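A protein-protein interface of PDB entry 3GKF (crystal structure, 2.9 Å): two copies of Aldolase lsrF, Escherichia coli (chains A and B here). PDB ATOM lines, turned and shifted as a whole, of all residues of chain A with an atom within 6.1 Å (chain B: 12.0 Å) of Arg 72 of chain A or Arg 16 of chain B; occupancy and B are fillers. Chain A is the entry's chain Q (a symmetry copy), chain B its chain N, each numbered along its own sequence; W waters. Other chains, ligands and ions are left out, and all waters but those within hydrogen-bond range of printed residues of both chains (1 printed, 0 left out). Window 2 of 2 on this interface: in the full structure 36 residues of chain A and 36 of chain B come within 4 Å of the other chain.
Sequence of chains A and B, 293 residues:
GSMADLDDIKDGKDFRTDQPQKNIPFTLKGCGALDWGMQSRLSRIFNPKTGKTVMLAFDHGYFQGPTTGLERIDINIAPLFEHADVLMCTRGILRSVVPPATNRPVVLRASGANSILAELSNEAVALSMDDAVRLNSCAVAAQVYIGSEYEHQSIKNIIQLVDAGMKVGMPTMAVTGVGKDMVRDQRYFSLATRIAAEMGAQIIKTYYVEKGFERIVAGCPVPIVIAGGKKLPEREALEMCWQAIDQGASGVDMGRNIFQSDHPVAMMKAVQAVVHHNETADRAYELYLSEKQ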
ATOM      1  N   GLY A  69     -26.203 -14.387   0.348  1.00  0.00           N
ATOM      2  CA  GLY A  69     -25.464 -15.574  -0.011  1.00  0.00           C
ATOM      3  C   GLY A  69     -25.135 -15.601  -1.488  1.00  0.00           C
ATOM      4  O   GLY A  69     -24.310 -16.395  -1.913  1.00  0.00           O
ATOM      5  N   LEU A  70     -25.799 -14.758  -2.275  1.00  0.00           N
ATOM      6  CA  LEU A  70     -25.499 -14.634  -3.700  1.00  0.00           C
ATOM      7  C   LEU A  70     -24.855 -13.294  -3.931  1.00  0.00           C
ATOM      8  O   LEU A  70     -24.789 -12.819  -5.054  1.00  0.00           O
ATOM      9  CB  LEU A  70     -26.764 -14.665  -4.531  1.00  0.00           C
ATOM     10  CG  LEU A  70     -27.821 -15.697  -4.132  1.00  0.00           C
ATOM     11  CD1 LEU A  70     -29.245 -15.130  -4.433  1.00  0.00           C
ATOM     12  CD2 LEU A  70     -27.571 -17.027  -4.814  1.00  0.00           C
ATOM     13  N   GLU A  71     -24.409 -12.664  -2.855  1.00  0.00           N
ATOM     14  CA  GLU A  71     -23.792 -11.362  -2.989  1.00  0.00           C
ATOM     15  C   GLU A  71     -22.638 -11.491  -3.966  1.00  0.00           C
ATOM     16  O   GLU A  71     -22.527 -10.748  -4.923  1.00  0.00           O
ATOM     17  CB  GLU A  71     -23.294 -10.834  -1.637  1.00  0.00           C
ATOM     18  CG  GLU A  71     -24.383 -10.613  -0.604  1.00  0.00           C
ATOM     19  CD  GLU A  71     -24.599 -11.806   0.291  1.00  0.00           C
ATOM     20  OE1 GLU A  71     -24.196 -12.931  -0.106  1.00  0.00           O
ATOM     21  OE2 GLU A  71     -25.160 -11.609   1.393  1.00  0.00           O
ATOM     22  N   ARG A  72     -21.771 -12.455  -3.716  1.00  0.00           N
ATOM     23  CA  ARG A  72     -20.619 -12.640  -4.564  1.00  0.00           C
ATOM     24  C   ARG A  72     -20.562 -14.077  -5.081  1.00  0.00           C
ATOM     25  O   ARG A  72     -19.932 -14.931  -4.464  1.00  0.00           O
ATOM     26  CB  ARG A  72     -19.341 -12.306  -3.802  1.00  0.00           C
ATOM     27  CG  ARG A  72     -19.247 -10.875  -3.364  1.00  0.00           C
ATOM     28  CD  ARG A  72     -18.713 -10.020  -4.469  1.00  0.00           C
ATOM     29  NE  ARG A  72     -17.505 -10.595  -5.022  1.00  0.00           N
ATOM     30  CZ  ARG A  72     -16.287 -10.121  -4.796  1.00  0.00           C
ATOM     31  NH1 ARG A  72     -16.143  -9.053  -4.041  1.00  0.00           N
ATOM     32  NH2 ARG A  72     -15.216 -10.706  -5.331  1.00  0.00           N
ATOM     33  N   ILE A  73     -21.224 -14.337  -6.207  1.00  0.00           N
ATOM     34  CA  ILE A  73     -21.199 -15.662  -6.761  1.00  0.00           C
ATOM     35  C   ILE A  73     -19.765 -16.090  -6.932  1.00  0.00           C
ATOM     36  O   ILE A  73     -19.422 -17.245  -6.655  1.00  0.00           O
ATOM     37  CB  ILE A  73     -21.837 -15.707  -8.132  1.00  0.00           C
ATOM     38  CG1 ILE A  73     -23.247 -15.108  -8.082  1.00  0.00           C
ATOM     39  CG2 ILE A  73     -21.836 -17.134  -8.655  1.00  0.00           C
ATOM     40  CD1 ILE A  73     -24.295 -15.977  -7.450  1.00  0.00           C
ATOM     41  N   ASP A  74     -18.932 -15.169  -7.405  1.00  0.00           N
ATOM     42  CA  ASP A  74     -17.590 -15.523  -7.853  1.00  0.00           C
ATOM     43  C   ASP A  74     -16.751 -16.115  -6.739  1.00  0.00           C
ATOM     44  O   ASP A  74     -15.827 -16.887  -6.978  1.00  0.00           O
ATOM     45  CB  ASP A  74     -16.869 -14.313  -8.421  1.00  0.00           C
ATOM     46  CG  ASP A  74     -16.911 -13.121  -7.481  1.00  0.00           C
ATOM     47  OD1 ASP A  74     -18.021 -12.728  -7.059  1.00  0.00           O
ATOM     48  OD2 ASP A  74     -15.834 -12.564  -7.183  1.00  0.00           O
ATOM     49  N   ILE A  75     -17.087 -15.755  -5.509  1.00  0.00           N
ATOM     50  CA  ILE A  75     -16.308 -16.171  -4.357  1.00  0.00           C
ATOM     51  C   ILE A  75     -17.030 -17.233  -3.555  1.00  0.00           C
ATOM     52  O   ILE A  75     -16.507 -18.303  -3.323  1.00  0.00           O
ATOM     53  CB  ILE A  75     -16.026 -14.959  -3.460  1.00  0.00           C
ATOM     54  CG1 ILE A  75     -14.728 -14.292  -3.899  1.00  0.00           C
ATOM     55  CG2 ILE A  75     -15.952 -15.383  -2.008  1.00  0.00           C
ATOM     56  CD1 ILE A  75     -14.689 -12.859  -3.618  1.00  0.00           C
ATOM     57  N   ASN A  76     -18.233 -16.913  -3.132  1.00  0.00           N
ATOM     58  CA  ASN A  76     -19.085 -17.811  -2.390  1.00  0.00           C
ATOM     59  C   ASN A  76     -19.479 -19.110  -3.089  1.00  0.00           C
ATOM     60  O   ASN A  76     -19.428 -20.176  -2.507  1.00  0.00           O
ATOM     61  CB  ASN A  76     -20.380 -17.082  -2.164  1.00  0.00           C
ATOM     62  CG  ASN A  76     -20.843 -17.182  -0.771  1.00  0.00           C
ATOM     63  OD1 ASN A  76     -20.155 -16.715   0.140  1.00  0.00           O
ATOM     64  ND2 ASN A  76     -22.032 -17.766  -0.570  1.00  0.00           N
ATOM     65  N   ILE A  77     -19.936 -18.996  -4.332  1.00  0.00           N
ATOM     66  CA  ILE A  77     -20.510 -20.121  -5.047  1.00  0.00           C
ATOM     67  C   ILE A  77     -19.480 -20.824  -5.927  1.00  0.00           C
ATOM     68  O   ILE A  77     -19.585 -22.023  -6.176  1.00  0.00           O
ATOM     69  CB  ILE A  77     -21.696 -19.659  -5.908  1.00  0.00           C
ATOM     70  CG1 ILE A  77     -22.680 -18.868  -5.056  1.00  0.00           C
ATOM     71  CG2 ILE A  77     -22.413 -20.852  -6.528  1.00  0.00           C
ATOM     72  CD1 ILE A  77     -23.461 -19.726  -4.116  1.00  0.00           C
ATOM     73  N   ALA A  78     -18.480 -20.089  -6.400  1.00  0.00           N
ATOM     74  CA  ALA A  78     -17.500 -20.692  -7.309  1.00  0.00           C
ATOM     75  C   ALA A  78     -16.941 -22.032  -6.806  1.00  0.00           C
ATOM     76  O   ALA A  78     -16.785 -22.955  -7.581  1.00  0.00           O
ATOM     77  CB  ALA A  78     -16.370 -19.711  -7.634  1.00  0.00           C
ATOM     78  N   GLY B  12     -27.603  -7.464   7.157  1.00  0.00           N
ATOM     79  CA  GLY B  12     -26.961  -8.796   7.371  1.00  0.00           C
ATOM     80  C   GLY B  12     -26.457  -9.444   6.086  1.00  0.00           C
ATOM     81  O   GLY B  12     -26.379 -10.673   5.978  1.00  0.00           O
ATOM     82  N   LYS B  13     -26.110  -8.615   5.102  1.00  0.00           N
ATOM     83  CA  LYS B  13     -25.614  -9.088   3.812  1.00  0.00           C
ATOM     84  C   LYS B  13     -24.124  -8.796   3.717  1.00  0.00           C
ATOM     85  O   LYS B  13     -23.674  -7.747   4.176  1.00  0.00           O
ATOM     86  CB  LYS B  13     -26.345  -8.376   2.669  1.00  0.00           C
ATOM     87  CG  LYS B  13     -27.507  -9.136   2.058  1.00  0.00           C
ATOM     88  CD  LYS B  13     -28.235  -8.275   1.036  1.00  0.00           C
ATOM     89  CE  LYS B  13     -29.678  -8.718   0.919  1.00  0.00           C
ATOM     90  NZ  LYS B  13     -30.506  -7.695   0.257  1.00  0.00           N
ATOM     91  N   ASP B  14     -23.359  -9.707   3.113  1.00  0.00           N
ATOM     92  CA  ASP B  14     -21.913  -9.485   2.925  1.00  0.00           C
ATOM     93  C   ASP B  14     -21.434  -9.466   1.465  1.00  0.00           C
ATOM     94  O   ASP B  14     -21.435 -10.492   0.792  1.00  0.00           O
ATOM     95  CB  ASP B  14     -21.103 -10.529   3.687  1.00  0.00           C
ATOM     96  CG  ASP B  14     -19.631 -10.181   3.753  1.00  0.00           C
ATOM     97  OD1 ASP B  14     -19.267  -9.028   3.434  1.00  0.00           O
ATOM     98  OD2 ASP B  14     -18.843 -11.060   4.137  1.00  0.00           O
ATOM     99  N   PHE B  15     -20.990  -8.303   0.993  1.00  0.00           N
ATOM    100  CA  PHE B  15     -20.551  -8.155  -0.395  1.00  0.00           C
ATOM    101  C   PHE B  15     -19.067  -8.332  -0.499  1.00  0.00           C
ATOM    102  O   PHE B  15     -18.504  -8.246  -1.575  1.00  0.00           O
ATOM    103  CB  PHE B  15     -20.954  -6.789  -0.966  1.00  0.00           C
ATOM    104  CG  PHE B  15     -22.438  -6.614  -1.104  1.00  0.00           C
ATOM    105  CD1 PHE B  15     -23.047  -6.680  -2.346  1.00  0.00           C
ATOM    106  CD2 PHE B  15     -23.223  -6.431   0.027  1.00  0.00           C
ATOM    107  CE1 PHE B  15     -24.404  -6.531  -2.454  1.00  0.00           C
ATOM    108  CE2 PHE B  15     -24.569  -6.295  -0.067  1.00  0.00           C
ATOM    109  CZ  PHE B  15     -25.171  -6.337  -1.305  1.00  0.00           C
ATOM    110  N   ARG B  16     -18.424  -8.570   0.629  1.00  0.00           N
ATOM    111  CA  ARG B  16     -17.007  -8.824   0.616  1.00  0.00           C
ATOM    112  C   ARG B  16     -16.309  -7.758  -0.205  1.00  0.00           C
ATOM    113  O   ARG B  16     -15.621  -8.052  -1.163  1.00  0.00           O
ATOM    114  CB  ARG B  16     -16.765 -10.175  -0.020  1.00  0.00           C
ATOM    115  CG  ARG B  16     -15.310 -10.505  -0.191  1.00  0.00           C
ATOM    116  CD  ARG B  16     -14.904 -11.482   0.886  1.00  0.00           C
ATOM    117  NE  ARG B  16     -16.079 -12.254   1.283  1.00  0.00           N
ATOM    118  CZ  ARG B  16     -16.040 -13.527   1.651  1.00  0.00           C
ATOM    119  NH1 ARG B  16     -14.877 -14.180   1.659  1.00  0.00           N
ATOM    120  NH2 ARG B  16     -17.160 -14.147   2.001  1.00  0.00           N
ATOM    121  N   THR B  17     -16.501  -6.506   0.176  1.00  0.00           N
ATOM    122  CA  THR B  17     -15.910  -5.382  -0.547  1.00  0.00           C
ATOM    123  C   THR B  17     -14.402  -5.365  -0.481  1.00  0.00           C
ATOM    124  O   THR B  17     -13.748  -4.778  -1.332  1.00  0.00           O
ATOM    125  CB  THR B  17     -16.388  -4.051   0.017  1.00  0.00           C
ATOM    126  OG1 THR B  17     -16.904  -4.268   1.325  1.00  0.00           O
ATOM    127  CG2 THR B  17     -17.488  -3.491  -0.849  1.00  0.00           C
ATOM    128  N   ASP B  18     -13.851  -5.983   0.554  1.00  0.00           N
ATOM    129  CA  ASP B  18     -12.420  -5.957   0.773  1.00  0.00           C
ATOM    130  C   ASP B  18     -11.750  -6.887  -0.217  1.00  0.00           C
ATOM    131  O   ASP B  18     -10.546  -6.816  -0.423  1.00  0.00           O
ATOM    132  CB  ASP B  18     -12.092  -6.357   2.207  1.00  0.00           C
ATOM    133  CG  ASP B  18     -12.639  -7.732   2.576  1.00  0.00           C
ATOM    134  OD1 ASP B  18     -13.781  -8.088   2.200  1.00  0.00           O
ATOM    135  OD2 ASP B  18     -11.915  -8.475   3.261  1.00  0.00           O
ATOM    136  N   GLN B  19     -12.548  -7.737  -0.856  1.00  0.00           N
ATOM    137  CA  GLN B  19     -12.035  -8.714  -1.801  1.00  0.00           C
ATOM    138  C   GLN B  19     -12.651  -8.510  -3.167  1.00  0.00           C
ATOM    139  O   GLN B  19     -13.831  -8.734  -3.352  1.00  0.00           O
ATOM    140  CB  GLN B  19     -12.372 -10.102  -1.300  1.00  0.00           C
ATOM    141  CG  GLN B  19     -11.276 -11.097  -1.527  1.00  0.00           C
ATOM    142  CD  GLN B  19     -11.729 -12.498  -1.244  1.00  0.00           C
ATOM    143  OE1 GLN B  19     -12.560 -12.725  -0.361  1.00  0.00           O
ATOM    144  NE2 GLN B  19     -11.198 -13.453  -1.998  1.00  0.00           N
ATOM    145  N   PRO B  20     -11.855  -8.080  -4.130  1.00  0.00           N
ATOM    146  CA  PRO B  20     -12.352  -7.682  -5.429  1.00  0.00           C
ATOM    147  C   PRO B  20     -12.429  -8.816  -6.440  1.00  0.00           C
ATOM    148  O   PRO B  20     -11.491  -9.582  -6.580  1.00  0.00           O
ATOM    149  CB  PRO B  20     -11.311  -6.668  -5.883  1.00  0.00           C
ATOM    150  CG  PRO B  20     -10.079  -7.179  -5.308  1.00  0.00           C
ATOM    151  CD  PRO B  20     -10.424  -7.818  -3.990  1.00  0.00           C
ATOM    152  N   GLN B  21     -13.545  -8.897  -7.157  1.00  0.00           N
ATOM    153  CA  GLN B  21     -13.744  -9.917  -8.183  1.00  0.00           C
ATOM    154  C   GLN B  21     -12.609  -9.950  -9.195  1.00  0.00           C
ATOM    155  O   GLN B  21     -12.166  -8.919  -9.687  1.00  0.00           O
ATOM    156  CB  GLN B  21     -15.066  -9.680  -8.883  1.00  0.00           C
ATOM    157  CG  GLN B  21     -15.223 -10.365 -10.192  1.00  0.00           C
ATOM    158  CD  GLN B  21     -16.558 -10.058 -10.772  1.00  0.00           C
ATOM    159  OE1 GLN B  21     -17.421  -9.577 -10.062  1.00  0.00           O
ATOM    160  NE2 GLN B  21     -16.747 -10.321 -12.062  1.00  0.00           N
ATOM    161  N   LYS B  22     -12.140 -11.159  -9.488  1.00  0.00           N
ATOM    162  CA  LYS B  22     -10.994 -11.367 -10.364  1.00  0.00           C
ATOM    163  C   LYS B  22     -11.348 -12.402 -11.407  1.00  0.00           C
ATOM    164  O   LYS B  22     -12.056 -13.356 -11.111  1.00  0.00           O
ATOM    165  CB  LYS B  22      -9.811 -11.858  -9.542  1.00  0.00           C
ATOM    166  CG  LYS B  22      -8.457 -11.408 -10.041  1.00  0.00           C
ATOM    167  CD  LYS B  22      -7.451 -11.439  -8.896  1.00  0.00           C
ATOM    168  CE  LYS B  22      -7.979 -10.629  -7.701  1.00  0.00           C
ATOM    169  NZ  LYS B  22      -7.974 -11.409  -6.413  1.00  0.00           N
ATOM    170  N   ASN B  23     -10.854 -12.217 -12.626  1.00  0.00           N
ATOM    171  CA  ASN B  23     -11.199 -13.123 -13.742  1.00  0.00           C
ATOM    172  C   ASN B  23     -10.346 -14.386 -13.804  1.00  0.00           C
ATOM    173  O   ASN B  23      -9.095 -14.311 -13.816  1.00  0.00           O
ATOM    174  CB  ASN B  23     -11.027 -12.419 -15.090  1.00  0.00           C
ATOM    175  CG  ASN B  23     -12.178 -11.540 -15.443  1.00  0.00           C
ATOM    176  OD1 ASN B  23     -13.167 -11.442 -14.715  1.00  0.00           O
ATOM    177  ND2 ASN B  23     -12.064 -10.886 -16.572  1.00  0.00           N
ATOM    178  N   ILE B  24     -11.003 -15.542 -13.895  1.00  0.00           N
ATOM    179  CA  ILE B  24     -10.240 -16.766 -14.046  1.00  0.00           C
ATOM    180  C   ILE B  24      -9.779 -16.955 -15.489  1.00  0.00           C
ATOM    181  O   ILE B  24     -10.584 -16.984 -16.416  1.00  0.00           O
ATOM    182  CB  ILE B  24     -10.998 -17.978 -13.621  1.00  0.00           C
ATOM    183  CG1 ILE B  24     -10.948 -18.120 -12.112  1.00  0.00           C
ATOM    184  CG2 ILE B  24     -10.321 -19.163 -14.190  1.00  0.00           C
ATOM    185  CD1 ILE B  24     -12.182 -17.627 -11.449  1.00  0.00           C
HETATM  186  O   HOH W   1     -13.174 -13.529  -7.447  1.00  0.00           O
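Glu 71 of chain A touches Lys 13 of chain B. Arg 72 of chain A touches Phe 15 of chain B (CG to O, 3.3 Å). C of Pro 20 of chain B touches NH2 of Arg 72 of chain A, 3.5 Å away. Asp 74 of chain A touches Gln 21 of chain B. Gln 19 of chain B touches Ile 75 of chain A.
The backbone carbonyl oxygen of Arg 16 of chain B lies within hydrogen-bond range of the guanidinium group of Arg 72 of chain A (3.1 Å). The backbone NH (N) of Asp 14 of chain B is in hydrogen-bond range of the side-chain carboxylate (OE2) of Glu 71 of chain A (3.1 Å). N of Gln 21 of chain B lies close to NH2 of Arg 72 of chain A (3.1 Å). O of Gln 19 of chain B is in hydrogen-bond range of NH1 of Arg 72 of chain A (2.4 Å).
Arg 72 of chain A touches just these residues of chain B: Phe 15 (3.3 Å), Arg 16 (3.1 Å), Gln 19 (2.4 Å), Pro 20 (3.5 Å) and Gln 21 (3.1 Å). Printed residues of chain A within 4 Å of Arg 16 of chain B: Arg 72 (3.1 Å). No residue of chain B comes within 4 Å of Gly 69 of chain A. Glu 71 of chain A touches two residues of chain B. No residue of chain B comes within 4 Å of Ile 73 of chain A. Asp 74 of chain A touches just one residue of chain B: Gln 21. No residue of chain B comes within 4 Å of Asn 76 of chain A. Printed residues of chain B within 4 Å of Ile 75 of chain A: Gln 19 (3.8 Å). Of the printed residues of chain A, Phe 15 of chain B touches Arg 72. Printed residues of chain A within 4 Å of Lys 13 of chain B: Glu 71 (3.5 Å). Printed residues of chain A within 4 Å of Pro 20 of chain B: Arg 72 (3.5 Å). Of the printed residues of chain A, Gln 21 of chain B touches Arg 72 and Asp 74. Ile 24 of chain B touches none of the printed residues of chain A. The nearest residue of chain B that does not touch Arg 72 of chain A is Asp 14 of chain B (4.7 Å). The nearest printed residue of chain A that does not touch Pro 20 of chain B is Asp 74 of chain A (5.1 Å).
Water W1 bridges OD2 of Asp 74 of chain A (2.8 Å) and N of Lys 22 of chain B (3.3 Å).
No position is printed for both chains. Of the 9 pairs that touch across the chains among the printed residues, none has its exchanged pair printed and touching as well.
N of Arg 16 of chain B sits at hydrogen-bond distance from OD1 of Asp 14 of chain B (3.0 Å). NH1 of Arg 16 of chain B sits close to OE1 of Gln 19 of chain B, at 3.4 Å. The guanidinium group (NH2) of Arg 72 of chain A is in salt-bridge range of the side-chain carboxylate (OD2) of Asp 74 of chain A. The side-chain carboxylate of Glu 71 of chain A lies within hydrogen-bond range of the backbone NH of Gly 69 of chain A, 2.5 Å away.
Of the 13 printed residues of chain B, 7 touch a printed residue of chain A. Printed residues of chain B that touch a printed residue of chain A: Lys 13, Asp 14, Phe 15, Arg 16, Gln 19, Pro 20 and Gln 21. Among the printed residues, 9 pairs touch across the chains. Among the printed residues, no Asp or Glu carboxylate lies within 4 Å of a Lys or Arg side-chain nitrogen of the other chain.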
